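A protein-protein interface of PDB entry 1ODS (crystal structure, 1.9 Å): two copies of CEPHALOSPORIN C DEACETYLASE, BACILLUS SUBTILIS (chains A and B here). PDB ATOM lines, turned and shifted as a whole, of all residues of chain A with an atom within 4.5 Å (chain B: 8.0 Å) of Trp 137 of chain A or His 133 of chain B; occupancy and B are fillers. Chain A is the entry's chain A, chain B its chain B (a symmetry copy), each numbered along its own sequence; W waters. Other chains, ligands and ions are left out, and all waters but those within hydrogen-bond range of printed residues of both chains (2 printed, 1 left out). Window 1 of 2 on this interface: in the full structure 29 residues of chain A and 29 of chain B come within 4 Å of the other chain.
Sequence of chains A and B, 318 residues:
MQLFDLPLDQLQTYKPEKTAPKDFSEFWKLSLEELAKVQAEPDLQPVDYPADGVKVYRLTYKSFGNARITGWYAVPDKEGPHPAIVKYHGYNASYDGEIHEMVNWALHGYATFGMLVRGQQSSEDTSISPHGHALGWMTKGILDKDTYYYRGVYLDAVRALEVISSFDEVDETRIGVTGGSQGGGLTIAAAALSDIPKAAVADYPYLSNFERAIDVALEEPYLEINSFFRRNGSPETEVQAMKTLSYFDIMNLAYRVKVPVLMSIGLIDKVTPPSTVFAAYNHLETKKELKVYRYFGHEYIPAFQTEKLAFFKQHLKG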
ATOM      1  N   TYR A  91      16.199  22.006 -11.874  1.00  0.00           N
ATOM      2  CA  TYR A  91      14.982  21.478 -12.502  1.00  0.00           C
ATOM      3  C   TYR A  91      14.079  20.820 -11.469  1.00  0.00           C
ATOM      4  O   TYR A  91      14.485  19.861 -10.789  1.00  0.00           O
ATOM      5  CB  TYR A  91      15.401  20.469 -13.569  1.00  0.00           C
ATOM      6  CG  TYR A  91      14.314  19.838 -14.416  1.00  0.00           C
ATOM      7  CD1 TYR A  91      13.946  20.388 -15.638  1.00  0.00           C
ATOM      8  CD2 TYR A  91      13.666  18.662 -14.003  1.00  0.00           C
ATOM      9  CE1 TYR A  91      12.968  19.814 -16.415  1.00  0.00           C
ATOM     10  CE2 TYR A  91      12.692  18.067 -14.789  1.00  0.00           C
ATOM     11  CZ  TYR A  91      12.349  18.658 -16.000  1.00  0.00           C
ATOM     12  OH  TYR A  91      11.381  18.090 -16.783  1.00  0.00           O
ATOM     13  N   ASN A  92      12.860  21.333 -11.329  1.00  0.00           N
ATOM     14  CA  ASN A  92      11.905  20.807 -10.352  1.00  0.00           C
ATOM     15  C   ASN A  92      12.446  20.845  -8.910  1.00  0.00           C
ATOM     16  O   ASN A  92      12.012  20.069  -8.060  1.00  0.00           O
ATOM     17  CB  ASN A  92      11.505  19.365 -10.733  1.00  0.00           C
ATOM     18  CG  ASN A  92      10.307  18.825  -9.940  1.00  0.00           C
ATOM     19  OD1 ASN A  92       9.250  19.451  -9.863  1.00  0.00           O
ATOM     20  ND2 ASN A  92      10.459  17.614  -9.395  1.00  0.00           N
ATOM     21  N   GLY A 119       6.348  27.632 -14.583  1.00  0.00           N
ATOM     22  CA  GLY A 119       5.744  26.318 -14.637  1.00  0.00           C
ATOM     23  C   GLY A 119       6.261  25.347 -13.589  1.00  0.00           C
ATOM     24  O   GLY A 119       5.582  24.369 -13.297  1.00  0.00           O
ATOM     25  N   GLN A 120       7.437  25.631 -13.026  1.00  0.00           N
ATOM     26  CA  GLN A 120       8.069  24.805 -11.999  1.00  0.00           C
ATOM     27  C   GLN A 120       7.778  25.239 -10.564  1.00  0.00           C
ATOM     28  O   GLN A 120       7.468  24.414  -9.723  1.00  0.00           O
ATOM     29  CB  GLN A 120       9.587  24.740 -12.209  1.00  0.00           C
ATOM     30  CG  GLN A 120       9.961  24.004 -13.494  1.00  0.00           C
ATOM     31  CD  GLN A 120      11.452  23.878 -13.768  1.00  0.00           C
ATOM     32  OE1 GLN A 120      11.868  23.846 -14.944  1.00  0.00           O
ATOM     33  NE2 GLN A 120      12.257  23.812 -12.727  1.00  0.00           N
ATOM     34  N   GLY A 136       7.073  15.711 -17.684  1.00  0.00           N
ATOM     35  CA  GLY A 136       8.092  16.713 -17.425  1.00  0.00           C
ATOM     36  C   GLY A 136       8.001  17.879 -18.374  1.00  0.00           C
ATOM     37  O   GLY A 136       7.020  17.979 -19.125  1.00  0.00           O
ATOM     38  N   TRP A 137       8.991  18.776 -18.295  1.00  0.00           N
ATOM     39  CA  TRP A 137       9.058  19.987 -19.114  1.00  0.00           C
ATOM     40  C   TRP A 137      10.022  19.863 -20.312  1.00  0.00           C
ATOM     41  O   TRP A 137       9.988  20.676 -21.235  1.00  0.00           O
ATOM     42  CB  TRP A 137       9.457  21.216 -18.259  1.00  0.00           C
ATOM     43  CG  TRP A 137       8.455  21.614 -17.203  1.00  0.00           C
ATOM     44  CD1 TRP A 137       7.355  22.426 -17.356  1.00  0.00           C
ATOM     45  CD2 TRP A 137       8.464  21.218 -15.837  1.00  0.00           C
ATOM     46  NE1 TRP A 137       6.683  22.550 -16.159  1.00  0.00           N
ATOM     47  CE2 TRP A 137       7.346  21.818 -15.209  1.00  0.00           C
ATOM     48  CE3 TRP A 137       9.300  20.408 -15.068  1.00  0.00           C
ATOM     49  CZ2 TRP A 137       7.050  21.622 -13.870  1.00  0.00           C
ATOM     50  CZ3 TRP A 137       9.007  20.229 -13.726  1.00  0.00           C
ATOM     51  CH2 TRP A 137       7.896  20.838 -13.138  1.00  0.00           C
ATOM     52  N   MET A 138      10.901  18.867 -20.281  1.00  0.00           N
ATOM     53  CA  MET A 138      11.992  18.775 -21.253  1.00  0.00           C
ATOM     54  C   MET A 138      11.543  18.635 -22.701  1.00  0.00           C
ATOM     55  O   MET A 138      12.271  19.038 -23.613  1.00  0.00           O
ATOM     56  CB  MET A 138      12.919  17.597 -20.929  1.00  0.00           C
ATOM     57  CG  MET A 138      13.729  17.736 -19.675  1.00  0.00           C
ATOM     58  SD  MET A 138      14.779  19.204 -19.633  1.00  0.00           S
ATOM     59  CE  MET A 138      15.776  19.010 -21.083  1.00  0.00           C
ATOM     60  N   THR A 139      10.374  18.040 -22.924  1.00  0.00           N
ATOM     61  CA  THR A 139       9.890  17.861 -24.278  1.00  0.00           C
ATOM     62  C   THR A 139       8.615  18.653 -24.613  1.00  0.00           C
ATOM     63  O   THR A 139       8.025  18.424 -25.674  1.00  0.00           O
ATOM     64  CB  THR A 139       9.723  16.364 -24.638  1.00  0.00           C
ATOM     65  OG1 THR A 139       8.852  15.677 -23.712  1.00  0.00           O
ATOM     66  CG2 THR A 139      11.084  15.653 -24.569  1.00  0.00           C
ATOM     67  N   LYS A 140       8.218  19.568 -23.715  1.00  0.00           N
ATOM     68  CA  LYS A 140       7.086  20.473 -23.930  1.00  0.00           C
ATOM     69  C   LYS A 140       7.429  21.438 -25.086  1.00  0.00           C
ATOM     70  O   LYS A 140       8.352  22.243 -24.989  1.00  0.00           O
ATOM     71  CB  LYS A 140       6.721  21.237 -22.639  1.00  0.00           C
ATOM     72  CG  LYS A 140       5.479  22.153 -22.690  1.00  0.00           C
ATOM     73  CD  LYS A 140       5.167  22.760 -21.298  1.00  0.00           C
ATOM     74  CE  LYS A 140       4.034  23.810 -21.339  1.00  0.00           C
ATOM     75  NZ  LYS A 140       4.465  25.100 -21.955  1.00  0.00           N
ATOM     76  N   TYR A 149       9.789  24.864 -24.545  1.00  0.00           N
ATOM     77  CA  TYR A 149       9.723  25.322 -23.146  1.00  0.00           C
ATOM     78  C   TYR A 149      10.852  26.273 -22.752  1.00  0.00           C
ATOM     79  O   TYR A 149      10.622  27.331 -22.150  1.00  0.00           O
ATOM     80  CB  TYR A 149       9.741  24.108 -22.226  1.00  0.00           C
ATOM     81  CG  TYR A 149       9.782  24.416 -20.745  1.00  0.00           C
ATOM     82  CD1 TYR A 149       8.693  25.014 -20.109  1.00  0.00           C
ATOM     83  CD2 TYR A 149      10.916  24.133 -19.986  1.00  0.00           C
ATOM     84  CE1 TYR A 149       8.727  25.324 -18.764  1.00  0.00           C
ATOM     85  CE2 TYR A 149      10.953  24.418 -18.615  1.00  0.00           C
ATOM     86  CZ  TYR A 149       9.858  25.010 -18.017  1.00  0.00           C
ATOM     87  OH  TYR A 149       9.877  25.292 -16.677  1.00  0.00           O
ATOM     88  N   GLU A 224      14.055  12.199 -20.174  1.00  0.00           N
ATOM     89  CA  GLU A 224      12.728  12.566 -20.664  1.00  0.00           C
ATOM     90  C   GLU A 224      12.702  12.621 -22.183  1.00  0.00           C
ATOM     91  O   GLU A 224      11.653  12.409 -22.796  1.00  0.00           O
ATOM     92  CB  GLU A 224      12.304  13.936 -20.135  1.00  0.00           C
ATOM     93  CG  GLU A 224      12.107  13.997 -18.646  1.00  0.00           C
ATOM     94  CD  GLU A 224      11.526  15.319 -18.189  1.00  0.00           C
ATOM     95  OE1 GLU A 224      11.029  16.084 -19.049  1.00  0.00           O
ATOM     96  OE2 GLU A 224      11.558  15.560 -16.959  1.00  0.00           O
ATOM     97  N   TYR B  91      -2.139   7.387 -17.752  1.00  0.00           N
ATOM     98  CA  TYR B  91      -1.317   8.576 -17.505  1.00  0.00           C
ATOM     99  C   TYR B  91       0.100   8.429 -18.079  1.00  0.00           C
ATOM    100  O   TYR B  91       0.848   7.525 -17.706  1.00  0.00           O
ATOM    101  CB  TYR B  91      -1.244   8.804 -15.999  1.00  0.00           C
ATOM    102  CG  TYR B  91      -0.594  10.077 -15.516  1.00  0.00           C
ATOM    103  CD1 TYR B  91       0.727  10.082 -15.116  1.00  0.00           C
ATOM    104  CD2 TYR B  91      -1.316  11.276 -15.437  1.00  0.00           C
ATOM    105  CE1 TYR B  91       1.336  11.226 -14.617  1.00  0.00           C
ATOM    106  CE2 TYR B  91      -0.723  12.445 -14.928  1.00  0.00           C
ATOM    107  CZ  TYR B  91       0.617  12.411 -14.526  1.00  0.00           C
ATOM    108  OH  TYR B  91       1.265  13.529 -14.023  1.00  0.00           O
ATOM    109  N   ILE B 128      -2.973  27.180 -19.657  1.00  0.00           N
ATOM    110  CA  ILE B 128      -1.640  27.532 -19.197  1.00  0.00           C
ATOM    111  C   ILE B 128      -1.245  26.855 -17.860  1.00  0.00           C
ATOM    112  O   ILE B 128      -2.009  26.059 -17.288  1.00  0.00           O
ATOM    113  CB  ILE B 128      -1.496  29.039 -19.120  1.00  0.00           C
ATOM    114  CG1 ILE B 128      -2.444  29.598 -18.077  1.00  0.00           C
ATOM    115  CG2 ILE B 128      -1.712  29.671 -20.502  1.00  0.00           C
ATOM    116  CD1 ILE B 128      -2.008  30.925 -17.596  1.00  0.00           C
ATOM    117  N   SER B 129      -0.034  27.159 -17.390  1.00  0.00           N
ATOM    118  CA  SER B 129       0.434  26.769 -16.047  1.00  0.00           C
ATOM    119  C   SER B 129       0.426  28.031 -15.174  1.00  0.00           C
ATOM    120  O   SER B 129       1.395  28.797 -15.187  1.00  0.00           O
ATOM    121  CB  SER B 129       1.854  26.182 -16.098  1.00  0.00           C
ATOM    122  OG  SER B 129       1.982  25.184 -17.095  1.00  0.00           O
ATOM    123  N   PRO B 130      -0.688  28.299 -14.490  1.00  0.00           N
ATOM    124  CA  PRO B 130      -0.870  29.579 -13.799  1.00  0.00           C
ATOM    125  C   PRO B 130       0.089  29.883 -12.644  1.00  0.00           C
ATOM    126  O   PRO B 130       0.359  31.058 -12.393  1.00  0.00           O
ATOM    127  CB  PRO B 130      -2.314  29.506 -13.246  1.00  0.00           C
ATOM    128  CG  PRO B 130      -2.808  28.114 -13.491  1.00  0.00           C
ATOM    129  CD  PRO B 130      -1.896  27.454 -14.448  1.00  0.00           C
ATOM    130  N   HIS B 131       0.562  28.852 -11.944  1.00  0.00           N
ATOM    131  CA  HIS B 131       1.242  29.057 -10.671  1.00  0.00           C
ATOM    132  C   HIS B 131       2.477  28.213 -10.403  1.00  0.00           C
ATOM    133  O   HIS B 131       3.109  28.387  -9.360  1.00  0.00           O
ATOM    134  CB  HIS B 131       0.266  28.842  -9.509  1.00  0.00           C
ATOM    135  CG  HIS B 131      -0.451  27.528  -9.535  1.00  0.00           C
ATOM    136  ND1 HIS B 131       0.184  26.336  -9.277  1.00  0.00           N
ATOM    137  CD2 HIS B 131      -1.759  27.225  -9.746  1.00  0.00           C
ATOM    138  CE1 HIS B 131      -0.697  25.349  -9.339  1.00  0.00           C
ATOM    139  NE2 HIS B 131      -1.882  25.864  -9.625  1.00  0.00           N
ATOM    140  N   GLY B 132       2.822  27.315 -11.316  1.00  0.00           N
ATOM    141  CA  GLY B 132       3.944  26.426 -11.107  1.00  0.00           C
ATOM    142  C   GLY B 132       3.494  25.182 -10.383  1.00  0.00           C
ATOM    143  O   GLY B 132       2.655  25.251  -9.466  1.00  0.00           O
ATOM    144  N   HIS B 133       4.041  24.043 -10.793  1.00  0.00           N
ATOM    145  CA  HIS B 133       3.554  22.751 -10.321  1.00  0.00           C
ATOM    146  C   HIS B 133       4.710  21.771 -10.193  1.00  0.00           C
ATOM    147  O   HIS B 133       5.800  21.992 -10.745  1.00  0.00           O
ATOM    148  CB  HIS B 133       2.427  22.226 -11.247  1.00  0.00           C
ATOM    149  CG  HIS B 133       2.857  21.986 -12.660  1.00  0.00           C
ATOM    150  ND1 HIS B 133       3.577  20.871 -13.031  1.00  0.00           N
ATOM    151  CD2 HIS B 133       2.647  22.697 -13.797  1.00  0.00           C
ATOM    152  CE1 HIS B 133       3.832  20.923 -14.325  1.00  0.00           C
ATOM    153  NE2 HIS B 133       3.265  22.014 -14.818  1.00  0.00           N
ATOM    154  N   ALA B 134       4.496  20.706  -9.422  1.00  0.00           N
ATOM    155  CA  ALA B 134       5.461  19.606  -9.343  1.00  0.00           C
ATOM    156  C   ALA B 134       5.518  18.880 -10.689  1.00  0.00           C
ATOM    157  O   ALA B 134       4.573  18.937 -11.488  1.00  0.00           O
ATOM    158  CB  ALA B 134       5.109  18.609  -8.220  1.00  0.00           C
ATOM    159  N   LEU B 135       6.654  18.240 -10.934  1.00  0.00           N
ATOM    160  CA  LEU B 135       6.902  17.453 -12.144  1.00  0.00           C
ATOM    161  C   LEU B 135       5.703  16.545 -12.434  1.00  0.00           C
ATOM    162  O   LEU B 135       5.333  15.751 -11.586  1.00  0.00           O
ATOM    163  CB  LEU B 135       8.152  16.585 -11.950  1.00  0.00           C
ATOM    164  CG  LEU B 135       8.513  15.585 -13.055  1.00  0.00           C
ATOM    165  CD1 LEU B 135       8.930  16.339 -14.238  1.00  0.00           C
ATOM    166  CD2 LEU B 135       9.630  14.612 -12.617  1.00  0.00           C
ATOM    167  N   GLY B 136       5.117  16.682 -13.621  1.00  0.00           N
ATOM    168  CA  GLY B 136       3.885  15.988 -14.006  1.00  0.00           C
ATOM    169  C   GLY B 136       2.739  16.919 -14.324  1.00  0.00           C
ATOM    170  O   GLY B 136       2.928  18.135 -14.316  1.00  0.00           O
ATOM    171  N   TRP B 137       1.564  16.356 -14.606  1.00  0.00           N
ATOM    172  CA  TRP B 137       0.340  17.113 -14.882  1.00  0.00           C
ATOM    173  C   TRP B 137      -0.612  17.189 -13.642  1.00  0.00           C
ATOM    174  O   TRP B 137      -1.539  18.002 -13.596  1.00  0.00           O
ATOM    175  CB  TRP B 137      -0.401  16.469 -16.079  1.00  0.00           C
ATOM    176  CG  TRP B 137       0.329  16.477 -17.406  1.00  0.00           C
ATOM    177  CD1 TRP B 137       0.279  17.461 -18.351  1.00  0.00           C
ATOM    178  CD2 TRP B 137       1.151  15.438 -17.963  1.00  0.00           C
ATOM    179  NE1 TRP B 137       1.057  17.123 -19.432  1.00  0.00           N
ATOM    180  CE2 TRP B 137       1.596  15.884 -19.225  1.00  0.00           C
ATOM    181  CE3 TRP B 137       1.578  14.178 -17.515  1.00  0.00           C
ATOM    182  CZ2 TRP B 137       2.428  15.128 -20.039  1.00  0.00           C
ATOM    183  CZ3 TRP B 137       2.424  13.435 -18.327  1.00  0.00           C
ATOM    184  CH2 TRP B 137       2.839  13.909 -19.571  1.00  0.00           C
ATOM    185  N   MET B 138      -0.422  16.299 -12.671  1.00  0.00           N
ATOM    186  CA  MET B 138      -1.340  16.178 -11.532  1.00  0.00           C
ATOM    187  C   MET B 138      -1.558  17.465 -10.751  1.00  0.00           C
ATOM    188  O   MET B 138      -2.597  17.656 -10.140  1.00  0.00           O
ATOM    189  CB  MET B 138      -0.869  15.095 -10.553  1.00  0.00           C
ATOM    190  CG  MET B 138      -0.925  13.692 -11.095  1.00  0.00           C
ATOM    191  SD  MET B 138      -2.516  13.210 -11.707  1.00  0.00           S
ATOM    192  CE  MET B 138      -3.515  13.290 -10.225  1.00  0.00           C
ATOM    193  N   THR B 139      -0.566  18.338 -10.723  1.00  0.00           N
ATOM    194  CA  THR B 139      -0.733  19.541  -9.942  1.00  0.00           C
ATOM    195  C   THR B 139      -0.716  20.793 -10.797  1.00  0.00           C
ATOM    196  O   THR B 139      -0.685  21.891 -10.263  1.00  0.00           O
ATOM    197  CB  THR B 139       0.281  19.615  -8.773  1.00  0.00           C
ATOM    198  OG1 THR B 139       1.644  19.549  -9.257  1.00  0.00           O
ATOM    199  CG2 THR B 139       0.082  18.417  -7.837  1.00  0.00           C
ATOM    200  N   LYS B 140      -0.804  20.613 -12.111  1.00  0.00           N
ATOM    201  CA  LYS B 140      -0.915  21.738 -13.054  1.00  0.00           C
ATOM    202  C   LYS B 140      -2.253  22.466 -12.846  1.00  0.00           C
ATOM    203  O   LYS B 140      -3.331  21.913 -13.066  1.00  0.00           O
ATOM    204  CB  LYS B 140      -0.739  21.248 -14.510  1.00  0.00           C
ATOM    205  CG  LYS B 140      -0.682  22.318 -15.577  1.00  0.00           C
ATOM    206  CD  LYS B 140      -0.315  21.750 -16.950  1.00  0.00           C
ATOM    207  CE  LYS B 140      -0.445  22.785 -18.064  1.00  0.00           C
ATOM    208  NZ  LYS B 140      -1.852  23.193 -18.349  1.00  0.00           N
ATOM    209  N   GLY B 141      -2.177  23.718 -12.406  1.00  0.00           N
ATOM    210  CA  GLY B 141      -3.376  24.533 -12.177  1.00  0.00           C
ATOM    211  C   GLY B 141      -4.223  24.146 -10.965  1.00  0.00           C
ATOM    212  O   GLY B 141      -5.396  24.537 -10.868  1.00  0.00           O
ATOM    213  N   ILE B 142      -3.629  23.377 -10.044  1.00  0.00           N
ATOM    214  CA  ILE B 142      -4.369  22.777  -8.911  1.00  0.00           C
ATOM    215  C   ILE B 142      -4.862  23.818  -7.896  1.00  0.00           C
ATOM    216  O   ILE B 142      -5.667  23.512  -7.025  1.00  0.00           O
ATOM    217  CB  ILE B 142      -3.495  21.673  -8.203  1.00  0.00           C
ATOM    218  CG1 ILE B 142      -4.342  20.694  -7.384  1.00  0.00           C
ATOM    219  CG2 ILE B 142      -2.403  22.331  -7.357  1.00  0.00           C
ATOM    220  CD1 ILE B 142      -3.595  19.490  -6.832  1.00  0.00           C
ATOM    221  N   TYR B 149      -5.777  21.028 -14.548  1.00  0.00           N
ATOM    222  CA  TYR B 149      -5.498  20.187 -15.717  1.00  0.00           C
ATOM    223  C   TYR B 149      -6.661  19.316 -16.162  1.00  0.00           C
ATOM    224  O   TYR B 149      -6.986  19.293 -17.362  1.00  0.00           O
ATOM    225  CB  TYR B 149      -4.296  19.289 -15.437  1.00  0.00           C
ATOM    226  CG  TYR B 149      -3.951  18.345 -16.569  1.00  0.00           C
ATOM    227  CD1 TYR B 149      -3.520  18.831 -17.804  1.00  0.00           C
ATOM    228  CD2 TYR B 149      -4.015  16.962 -16.395  1.00  0.00           C
ATOM    229  CE1 TYR B 149      -3.212  17.961 -18.847  1.00  0.00           C
ATOM    230  CE2 TYR B 149      -3.696  16.104 -17.416  1.00  0.00           C
ATOM    231  CZ  TYR B 149      -3.298  16.611 -18.640  1.00  0.00           C
ATOM    232  OH  TYR B 149      -2.957  15.766 -19.652  1.00  0.00           O
ATOM    233  N   GLU B 224       2.660  12.819  -6.909  1.00  0.00           N
ATOM    234  CA  GLU B 224       2.988  14.149  -7.417  1.00  0.00           C
ATOM    235  C   GLU B 224       2.331  15.205  -6.524  1.00  0.00           C
ATOM    236  O   GLU B 224       2.839  16.317  -6.368  1.00  0.00           O
ATOM    237  CB  GLU B 224       2.499  14.351  -8.860  1.00  0.00           C
ATOM    238  CG  GLU B 224       3.176  13.494  -9.916  1.00  0.00           C
ATOM    239  CD  GLU B 224       2.693  13.805 -11.314  1.00  0.00           C
ATOM    240  OE1 GLU B 224       2.061  14.879 -11.514  1.00  0.00           O
ATOM    241  OE2 GLU B 224       2.946  12.962 -12.219  1.00  0.00           O
ATOM    242  N   SER B 227       4.509  15.658  -3.707  1.00  0.00           N
ATOM    243  CA  SER B 227       5.685  16.402  -4.173  1.00  0.00           C
ATOM    244  C   SER B 227       5.394  17.907  -4.249  1.00  0.00           C
ATOM    245  O   SER B 227       6.224  18.712  -3.858  1.00  0.00           O
ATOM    246  CB  SER B 227       6.137  15.873  -5.539  1.00  0.00           C
ATOM    247  OG  SER B 227       6.636  14.538  -5.404  1.00  0.00           O
ATOM    248  N   PHE B 228       4.204  18.275  -4.718  1.00  0.00           N
ATOM    249  CA  PHE B 228       3.777  19.676  -4.817  1.00  0.00           C
ATOM    250  C   PHE B 228       3.727  20.344  -3.434  1.00  0.00           C
ATOM    251  O   PHE B 228       4.210  21.469  -3.246  1.00  0.00           O
ATOM    252  CB  PHE B 228       2.420  19.750  -5.534  1.00  0.00           C
ATOM    253  CG  PHE B 228       1.851  21.139  -5.643  1.00  0.00           C
ATOM    254  CD1 PHE B 228       2.330  22.038  -6.591  1.00  0.00           C
ATOM    255  CD2 PHE B 228       0.831  21.534  -4.806  1.00  0.00           C
ATOM    256  CE1 PHE B 228       1.774  23.321  -6.682  1.00  0.00           C
ATOM    257  CE2 PHE B 228       0.269  22.790  -4.891  1.00  0.00           C
ATOM    258  CZ  PHE B 228       0.727  23.691  -5.821  1.00  0.00           C
ATOM    259  N   ARG B 231       7.082  21.210  -2.090  1.00  0.00           N
ATOM    260  CA  ARG B 231       7.644  22.375  -2.794  1.00  0.00           C
ATOM    261  C   ARG B 231       6.884  23.692  -2.530  1.00  0.00           C
ATOM    262  O   ARG B 231       7.382  24.777  -2.843  1.00  0.00           O
ATOM    263  CB  ARG B 231       7.703  22.088  -4.300  1.00  0.00           C
ATOM    264  CG  ARG B 231       8.767  21.044  -4.690  1.00  0.00           C
ATOM    265  CD  ARG B 231       8.590  20.402  -6.056  1.00  0.00           C
ATOM    266  NE  ARG B 231       9.723  19.539  -6.358  1.00  0.00           N
ATOM    267  CZ  ARG B 231       9.952  18.349  -5.811  1.00  0.00           C
ATOM    268  NH1 ARG B 231       9.117  17.844  -4.909  1.00  0.00           N
ATOM    269  NH2 ARG B 231      11.031  17.655  -6.161  1.00  0.00           N
ATOM    270  N   ASN B 232       5.670  23.584  -2.003  1.00  0.00           N
ATOM    271  CA  ASN B 232       4.770  24.713  -1.753  1.00  0.00           C
ATOM    272  C   ASN B 232       4.070  24.447  -0.398  1.00  0.00           C
ATOM    273  O   ASN B 232       2.945  23.953  -0.341  1.00  0.00           O
ATOM    274  CB  ASN B 232       3.732  24.844  -2.878  1.00  0.00           C
ATOM    275  CG  ASN B 232       4.362  24.925  -4.266  1.00  0.00           C
ATOM    276  OD1 ASN B 232       4.536  26.037  -4.816  1.00  0.00           O
ATOM    277  ND2 ASN B 232       4.688  23.763  -4.854  1.00  0.00           N
HETATM  278  O   HOH W   1       4.912  24.716 -17.556  1.00  0.00           O
HETATM  279  O   HOH W   2       5.521  23.761  -7.690  1.00  0.00           O
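The side-chain amide oxygen (OD1) of Asn 92 of chain A lies within hydrogen-bond range of the backbone NH (N) of Leu 135 of chain B, 3.1 Å away.
O of Gly 119 of chain A is in hydrogen-bond range of N of His 133 of chain B.
The guanidinium group (NE) of Arg 231 of chain B is in hydrogen-bond range of the backbone carbonyl oxygen (O) of Asn 92 of chain A (2.9 Å).
O of Gln 120 of chain A sits close to O of His 133 of chain B (3.1 Å).
The side-chain carboxylate (OE1) of Glu 224 of chain A is in hydrogen-bond range of the backbone NH (N) of Trp 137 of chain A (3.5 Å).
A ring nitrogen (ND1) of His 133 of chain B sits close to the backbone carbonyl oxygen (O) of Gly 136 of chain B (3.1 Å).
The backbone NH (N) of Asn 92 of chain A sits close to the side-chain amide nitrogen (NE2) of Gln 120 of chain A (2.9 Å).
The side-chain hydroxyl (OH) of Tyr 91 of chain A is in hydrogen-bond range of the side-chain carboxylate (OE2) of Glu 224 of chain A, 2.5 Å away.
The side-chain amide oxygen (OE1) of Gln 120 of chain A is in hydrogen-bond range of the side-chain hydroxyl (OH) of Tyr 149 of chain A (3.0 Å).
The backbone NH (N) of Trp 137 of chain A lies within hydrogen-bond range of the side-chain hydroxyl (OH) of Tyr 91 of chain A, at 2.9 Å.
Leu 135 of chain B touches Tyr 91 of chain A.
OD1 of Asn 92 of chain A touches CA of Ala 134 of chain B (3.8 Å).
Gly 132 of chain B touches Gly 119 of chain A.
Gly 136 of chain A touches Leu 135 of chain B (CA to CD1, 3.3 Å).
His 133 of chain B touches Trp 137 of chain A (CE1 to CZ2, 3.3 Å).
Ala 134 of chain B touches Trp 137 of chain A (C to CH2, 3.9 Å).
Leu 135 of chain B touches Trp 137 of chain A (N to CH2, 3.6 Å).
Glu 224 of chain A touches Leu 135 of chain B.
Trp 137 of chain A touches just these residues of chain B: His 133 (3.3 Å), Ala 134 (3.9 Å) and Leu 135 (3.6 Å).
His 133 of chain B touches three residues of chain A.
Of the printed residues of chain B, Glu 224 of chain A touches Leu 135.
Of the printed residues of chain A, Leu 135 of chain B touches Tyr 91 (3.9 Å), Asn 92 (3.1 Å), Gly 136 (3.3 Å), Trp 137 (3.6 Å) and Glu 224 (3.9 Å).
Printed residues of chain B within 4 Å of Gly 119 of chain A: Gly 132 and His 133.
Printed residues of chain A within 4 Å of Ala 134 of chain B: Asn 92 and Trp 137.
Glu 224 of chain B touches none of the printed residues of chain A.
The nearest residue of chain B that does not touch Trp 137 of chain A is Gly 136 of chain B (5.0 Å).
Hydrophobic or aromatic side chains of chain A within 4 Å of the printed part of chain B: Tyr 91 and Trp 137.
Positions printed for both chains: 91, 136, 137, 138, 139, 140, 149 and 224.
Water W2 lies within hydrogen-bond range of the backbone carbonyl oxygen of Gln 120 of chain A (2.9 Å), the side-chain amide nitrogen of Asn 232 of chain B (3.0 Å) and the backbone NH of His 133 of chain B (3.4 Å).
Water W1 bridges the side-chain hydroxyl of Ser 129 of chain B (3.0 Å) and the indole nitrogen of Trp 137 of chain A (3.1 Å).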
